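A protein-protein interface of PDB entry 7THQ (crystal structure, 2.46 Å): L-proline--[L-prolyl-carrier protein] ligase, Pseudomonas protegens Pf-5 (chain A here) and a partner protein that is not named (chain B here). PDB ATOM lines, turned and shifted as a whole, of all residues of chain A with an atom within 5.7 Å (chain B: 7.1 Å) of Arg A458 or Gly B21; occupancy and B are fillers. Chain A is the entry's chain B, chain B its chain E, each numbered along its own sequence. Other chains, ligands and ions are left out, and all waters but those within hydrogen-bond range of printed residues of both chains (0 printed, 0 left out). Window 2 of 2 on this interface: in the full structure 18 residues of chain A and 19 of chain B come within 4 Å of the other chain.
The side-chain hydroxyl (OG1) of Thr B26 lies within hydrogen-bond range of the backbone carbonyl oxygen (O) of Asp B23, 3.0 Å away.
Among the printed residues, merely in contact across the chains: Leu A453 with Leu B15 (3.5 Å), Ile A454 with Leu B15 (3.7 Å), Lys A457 with Leu B31 (3.1 Å), Arg A458 with Gly B21 (3.9 Å), Arg A458 with Thr B26 (3.4 Å) and Ala A461 with Glu B30 (3.9 Å).
Printed residues of chain B within 4 Å of Arg A458: Gly B21 and Thr B26.
Gly B21 touches one residue of chain A.
Of the printed residues of chain B, Leu A453 touches Leu B15.
Of the printed residues of chain B, Ile A454 touches Leu B15 (3.7 Å).
Lys B19 touches none of the printed residues of chain A.
His A459 touches none of the printed residues of chain B.
Of the 13 printed residues of chain B, 5 touch a printed residue of chain A.
Hydrophobic or aromatic side chains of chain B that line the printed part of chain A: Leu B15.
Along chain B the printed residues that touch a printed residue of chain A span positions 15 to 31.
Hydrophobic or aromatic side chains of chain A that line the printed part of chain B: Leu A453, Ile A454 and Ala A461.
Among the printed residues, 6 pairs touch across the chains.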
ATOM      1  N   LEU A 453      25.044  -9.869   1.917  1.00  0.00           N
ATOM      2  CA  LEU A 453      24.410 -11.051   1.354  1.00  0.00           C
ATOM      3  C   LEU A 453      22.928 -10.806   1.109  1.00  0.00           C
ATOM      4  O   LEU A 453      22.392 -11.266   0.100  1.00  0.00           O
ATOM      5  CB  LEU A 453      24.638 -12.262   2.264  1.00  0.00           C
ATOM      6  CG  LEU A 453      24.030 -13.581   1.783  1.00  0.00           C
ATOM      7  CD1 LEU A 453      24.470 -13.860   0.355  1.00  0.00           C
ATOM      8  CD2 LEU A 453      24.429 -14.743   2.682  1.00  0.00           C
ATOM      9  N   ILE A 454      22.275 -10.005   1.957  1.00  0.00           N
ATOM     10  CA  ILE A 454      20.864  -9.690   1.739  1.00  0.00           C
ATOM     11  C   ILE A 454      20.692  -8.766   0.537  1.00  0.00           C
ATOM     12  O   ILE A 454      19.802  -8.977  -0.296  1.00  0.00           O
ATOM     13  CB  ILE A 454      20.242  -9.086   3.012  1.00  0.00           C
ATOM     14  CG1 ILE A 454      19.764 -10.199   3.945  1.00  0.00           C
ATOM     15  CG2 ILE A 454      19.084  -8.162   2.661  1.00  0.00           C
ATOM     16  N   ASP A 455      21.541  -7.740   0.415  1.00  0.00           N
ATOM     17  CA  ASP A 455      21.474  -6.875  -0.761  1.00  0.00           C
ATOM     18  C   ASP A 455      21.714  -7.677  -2.033  1.00  0.00           C
ATOM     19  O   ASP A 455      21.082  -7.423  -3.066  1.00  0.00           O
ATOM     20  CB  ASP A 455      22.486  -5.733  -0.648  1.00  0.00           C
ATOM     21  CG  ASP A 455      22.355  -4.711  -1.774  1.00  0.00           C
ATOM     22  OD1 ASP A 455      23.214  -3.810  -1.868  1.00  0.00           O
ATOM     23  OD2 ASP A 455      21.388  -4.797  -2.560  1.00  0.00           O
ATOM     24  N   LEU A 456      22.607  -8.665  -1.972  1.00  0.00           N
ATOM     25  CA  LEU A 456      22.817  -9.529  -3.125  1.00  0.00           C
ATOM     26  C   LEU A 456      21.596 -10.397  -3.408  1.00  0.00           C
ATOM     27  O   LEU A 456      21.302 -10.681  -4.575  1.00  0.00           O
ATOM     28  CB  LEU A 456      24.056 -10.401  -2.911  1.00  0.00           C
ATOM     29  CG  LEU A 456      25.300 -10.065  -3.740  1.00  0.00           C
ATOM     30  CD2 LEU A 456      26.529 -10.734  -3.148  1.00  0.00           C
ATOM     31  N   LYS A 457      20.870 -10.825  -2.367  1.00  0.00           N
ATOM     32  CA  LYS A 457      19.698 -11.674  -2.589  1.00  0.00           C
ATOM     33  C   LYS A 457      18.510 -10.886  -3.129  1.00  0.00           C
ATOM     34  O   LYS A 457      17.781 -11.384  -3.993  1.00  0.00           O
ATOM     35  CB  LYS A 457      19.308 -12.407  -1.301  1.00  0.00           C
ATOM     36  CG  LYS A 457      20.437 -13.200  -0.680  1.00  0.00           C
ATOM     37  CD  LYS A 457      19.976 -14.268   0.294  1.00  0.00           C
ATOM     38  CE  LYS A 457      21.135 -15.202   0.600  1.00  0.00           C
ATOM     39  NZ  LYS A 457      20.805 -16.319   1.520  1.00  0.00           N
ATOM     40  N   ARG A 458      18.290  -9.659  -2.642  1.00  0.00           N
ATOM     41  CA  ARG A 458      17.243  -8.837  -3.243  1.00  0.00           C
ATOM     42  C   ARG A 458      17.539  -8.577  -4.710  1.00  0.00           C
ATOM     43  O   ARG A 458      16.644  -8.660  -5.558  1.00  0.00           O
ATOM     44  CB  ARG A 458      17.083  -7.506  -2.511  1.00  0.00           C
ATOM     45  CG  ARG A 458      16.676  -7.599  -1.069  1.00  0.00           C
ATOM     46  CD  ARG A 458      16.429  -6.208  -0.527  1.00  0.00           C
ATOM     47  NE  ARG A 458      16.325  -6.221   0.924  1.00  0.00           N
ATOM     48  CZ  ARG A 458      15.208  -6.485   1.589  1.00  0.00           C
ATOM     49  NH1 ARG A 458      14.067  -6.651   0.935  1.00  0.00           N
ATOM     50  NH2 ARG A 458      15.215  -6.485   2.913  1.00  0.00           N
ATOM     51  N   HIS A 459      18.800  -8.273  -5.025  1.00  0.00           N
ATOM     52  CA  HIS A 459      19.191  -8.033  -6.408  1.00  0.00           C
ATOM     53  C   HIS A 459      18.920  -9.261  -7.267  1.00  0.00           C
ATOM     54  O   HIS A 459      18.400  -9.145  -8.383  1.00  0.00           O
ATOM     55  CB  HIS A 459      20.668  -7.638  -6.459  1.00  0.00           C
ATOM     56  CG  HIS A 459      21.204  -7.445  -7.844  1.00  0.00           C
ATOM     57  ND1 HIS A 459      20.928  -6.326  -8.600  1.00  0.00           N
ATOM     58  CD2 HIS A 459      22.013  -8.222  -8.602  1.00  0.00           C
ATOM     59  CE1 HIS A 459      21.536  -6.426  -9.768  1.00  0.00           C
ATOM     60  NE2 HIS A 459      22.201  -7.567  -9.796  1.00  0.00           N
ATOM     61  N   CYS A 460      19.264 -10.447  -6.760  1.00  0.00           N
ATOM     62  CA  CYS A 460      18.985 -11.679  -7.493  1.00  0.00           C
ATOM     63  C   CYS A 460      17.487 -11.933  -7.601  1.00  0.00           C
ATOM     64  O   CYS A 460      17.004 -12.390  -8.645  1.00  0.00           O
ATOM     65  CB  CYS A 460      19.676 -12.860  -6.812  1.00  0.00           C
ATOM     66  SG  CYS A 460      21.461 -12.957  -7.081  1.00  0.00           S
ATOM     67  N   ALA A 461      16.733 -11.629  -6.540  1.00  0.00           N
ATOM     68  CA  ALA A 461      15.301 -11.910  -6.531  1.00  0.00           C
ATOM     69  C   ALA A 461      14.558 -11.131  -7.605  1.00  0.00           C
ATOM     70  O   ALA A 461      13.476 -11.552  -8.027  1.00  0.00           O
ATOM     71  CB  ALA A 461      14.709 -11.595  -5.156  1.00  0.00           C
ATOM     72  N   GLN A 462      15.116 -10.005  -8.054  1.00  0.00           N
ATOM     73  CA  GLN A 462      14.515  -9.244  -9.141  1.00  0.00           C
ATOM     74  C   GLN A 462      14.701  -9.917 -10.494  1.00  0.00           C
ATOM     75  O   GLN A 462      13.965  -9.597 -11.433  1.00  0.00           O
ATOM     76  CB  GLN A 462      15.111  -7.835  -9.181  1.00  0.00           C
ATOM     77  CG  GLN A 462      14.768  -6.978  -7.979  1.00  0.00           C
ATOM     78  CD  GLN A 462      13.274  -6.823  -7.787  1.00  0.00           C
ATOM     79  OE1 GLN A 462      12.715  -7.255  -6.779  1.00  0.00           O
ATOM     80  NE2 GLN A 462      12.617  -6.202  -8.760  1.00  0.00           N
ATOM     81  N   ARG A 463      15.662 -10.832 -10.616  1.00  0.00           N
ATOM     82  CA  ARG A 463      15.998 -11.452 -11.891  1.00  0.00           C
ATOM     83  C   ARG A 463      15.722 -12.946 -11.948  1.00  0.00           C
ATOM     84  O   ARG A 463      15.457 -13.468 -13.032  1.00  0.00           O
ATOM     85  CB  ARG A 463      17.481 -11.229 -12.213  1.00  0.00           C
ATOM     86  CG  ARG A 463      17.830  -9.822 -12.657  1.00  0.00           C
ATOM     87  CD  ARG A 463      19.173  -9.395 -12.085  1.00  0.00           C
ATOM     88  NE  ARG A 463      19.314  -7.944 -12.045  1.00  0.00           N
ATOM     89  CZ  ARG A 463      19.723  -7.206 -13.072  1.00  0.00           C
ATOM     90  NH1 ARG A 463      20.030  -7.786 -14.225  1.00  0.00           N
ATOM     91  NH2 ARG A 463      19.823  -5.890 -12.950  1.00  0.00           N
ATOM     92  N   LEU B  15      22.566 -16.556   7.369  1.00  0.00           N
ATOM     93  CA  LEU B  15      23.267 -15.414   6.793  1.00  0.00           C
ATOM     94  C   LEU B  15      24.720 -15.399   7.237  1.00  0.00           C
ATOM     95  O   LEU B  15      25.430 -14.414   6.998  1.00  0.00           O
ATOM     96  CB  LEU B  15      22.576 -14.102   7.185  1.00  0.00           C
ATOM     97  CG  LEU B  15      21.490 -13.563   6.248  1.00  0.00           C
ATOM     98  CD1 LEU B  15      20.902 -12.261   6.772  1.00  0.00           C
ATOM     99  CD2 LEU B  15      22.019 -13.370   4.843  1.00  0.00           C
ATOM    100  N   GLU B  18      25.393 -12.377   9.644  1.00  0.00           N
ATOM    101  CA  GLU B  18      25.325 -10.997   9.156  1.00  0.00           C
ATOM    102  C   GLU B  18      23.895 -10.475   9.279  1.00  0.00           C
ATOM    103  O   GLU B  18      23.061 -10.701   8.400  1.00  0.00           O
ATOM    104  CB  GLU B  18      25.827 -10.908   7.719  1.00  0.00           C
ATOM    105  N   LYS B  19      23.628  -9.741  10.359  1.00  0.00           N
ATOM    106  CA  LYS B  19      22.322  -9.165  10.666  1.00  0.00           C
ATOM    107  C   LYS B  19      22.073  -7.832   9.962  1.00  0.00           C
ATOM    108  O   LYS B  19      21.131  -7.124  10.333  1.00  0.00           O
ATOM    109  CB  LYS B  19      22.169  -8.987  12.180  1.00  0.00           C
ATOM    110  N   ASP B  20      22.895  -7.483   8.970  1.00  0.00           N
ATOM    111  CA  ASP B  20      22.876  -6.147   8.379  1.00  0.00           C
ATOM    112  C   ASP B  20      21.506  -5.757   7.826  1.00  0.00           C
ATOM    113  O   ASP B  20      20.953  -4.714   8.190  1.00  0.00           O
ATOM    114  CB  ASP B  20      23.933  -6.068   7.273  1.00  0.00           C
ATOM    115  N   GLY B  21      20.943  -6.578   6.943  1.00  0.00           N
ATOM    116  CA  GLY B  21      19.704  -6.224   6.272  1.00  0.00           C
ATOM    117  C   GLY B  21      18.436  -6.914   6.738  1.00  0.00           C
ATOM    118  O   GLY B  21      17.358  -6.668   6.187  1.00  0.00           O
ATOM    119  N   LEU B  22      18.539  -7.756   7.759  1.00  0.00           N
ATOM    120  CA  LEU B  22      17.421  -8.580   8.194  1.00  0.00           C
ATOM    121  C   LEU B  22      16.579  -7.872   9.247  1.00  0.00           C
ATOM    122  O   LEU B  22      17.106  -7.229  10.160  1.00  0.00           O
ATOM    123  CB  LEU B  22      17.923  -9.915   8.749  1.00  0.00           C
ATOM    124  N   ASP B  23      15.261  -7.984   9.094  1.00  0.00           N
ATOM    125  CA  ASP B  23      14.336  -7.505  10.108  1.00  0.00           C
ATOM    126  C   ASP B  23      13.094  -8.380  10.116  1.00  0.00           C
ATOM    127  O   ASP B  23      12.941  -9.310   9.317  1.00  0.00           O
ATOM    128  CB  ASP B  23      13.955  -6.022   9.909  1.00  0.00           C
ATOM    129  CG  ASP B  23      13.008  -5.772   8.715  1.00  0.00           C
ATOM    130  OD1 ASP B  23      13.206  -4.748   8.029  1.00  0.00           O
ATOM    131  OD2 ASP B  23      12.056  -6.537   8.464  1.00  0.00           O
ATOM    132  N   GLN B  25      10.235  -7.956   9.047  1.00  0.00           N
ATOM    133  CA  GLN B  25       9.349  -7.927   7.880  1.00  0.00           C
ATOM    134  C   GLN B  25       9.964  -8.424   6.571  1.00  0.00           C
ATOM    135  O   GLN B  25       9.238  -8.521   5.576  1.00  0.00           O
ATOM    136  CB  GLN B  25       8.802  -6.508   7.660  1.00  0.00           C
ATOM    137  CG  GLN B  25       8.147  -5.900   8.887  1.00  0.00           C
ATOM    138  N   THR B  26      11.261  -8.724   6.529  1.00  0.00           N
ATOM    139  CA  THR B  26      11.890  -9.210   5.299  1.00  0.00           C
ATOM    140  C   THR B  26      11.323 -10.566   4.877  1.00  0.00           C
ATOM    141  O   THR B  26      11.195 -11.467   5.718  1.00  0.00           O
ATOM    142  CB  THR B  26      13.405  -9.318   5.464  1.00  0.00           C
ATOM    143  OG1 THR B  26      13.711 -10.205   6.548  1.00  0.00           O
ATOM    144  CG2 THR B  26      14.017  -7.950   5.724  1.00  0.00           C
ATOM    145  N   PRO B  27      10.973 -10.754   3.601  1.00  0.00           N
ATOM    146  CA  PRO B  27      10.433 -12.050   3.152  1.00  0.00           C
ATOM    147  C   PRO B  27      11.537 -13.095   3.081  1.00  0.00           C
ATOM    148  O   PRO B  27      12.486 -12.961   2.307  1.00  0.00           O
ATOM    149  CB  PRO B  27       9.876 -11.738   1.757  1.00  0.00           C
ATOM    150  CG  PRO B  27       9.765 -10.248   1.696  1.00  0.00           C
ATOM    151  CD  PRO B  27      10.894  -9.739   2.540  1.00  0.00           C
ATOM    152  N   GLU B  30      11.094 -15.609  -0.385  1.00  0.00           N
ATOM    153  CA  GLU B  30      11.338 -14.902  -1.639  1.00  0.00           C
ATOM    154  C   GLU B  30      12.816 -14.587  -1.823  1.00  0.00           C
ATOM    155  O   GLU B  30      13.290 -14.474  -2.958  1.00  0.00           O
ATOM    156  CB  GLU B  30      10.530 -13.606  -1.684  1.00  0.00           C
ATOM    157  CG  GLU B  30       9.042 -13.761  -1.446  1.00  0.00           C
ATOM    158  CD  GLU B  30       8.304 -12.450  -1.629  1.00  0.00           C
ATOM    159  OE1 GLU B  30       8.873 -11.395  -1.279  1.00  0.00           O
ATOM    160  OE2 GLU B  30       7.157 -12.470  -2.122  1.00  0.00           O
ATOM    161  N   LEU B  31      13.554 -14.450  -0.725  1.00  0.00           N
ATOM    162  CA  LEU B  31      14.971 -14.118  -0.761  1.00  0.00           C
ATOM    163  C   LEU B  31      15.866 -15.336  -0.577  1.00  0.00           C
ATOM    164  O   LEU B  31      17.081 -15.177  -0.427  1.00  0.00           O
ATOM    165  CB  LEU B  31      15.286 -13.083   0.319  1.00  0.00           C
ATOM    166  CG  LEU B  31      15.262 -11.599  -0.041  1.00  0.00           C
ATOM    167  CD1 LEU B  31      13.952 -11.224  -0.711  1.00  0.00           C
ATOM    168  CD2 LEU B  31      15.481 -10.759   1.209  1.00  0.00           C
ATOM    169  N   ILE B  33      16.541 -16.932   1.840  1.00  0.00           N
ATOM    170  CA  ILE B  33      17.195 -17.002   3.142  1.00  0.00           C
ATOM    171  C   ILE B  33      16.889 -18.339   3.800  1.00  0.00           C
ATOM    172  O   ILE B  33      17.785 -19.034   4.292  1.00  0.00           O
ATOM    173  CB  ILE B  33      16.758 -15.829   4.037  1.00  0.00           C
ATOM    174  CG1 ILE B  33      17.103 -14.484   3.398  1.00  0.00           C
ATOM    175  CG2 ILE B  33      17.397 -15.953   5.415  1.00  0.00           C
ATOM    176  CD1 ILE B  33      16.100 -13.398   3.726  1.00  0.00           C
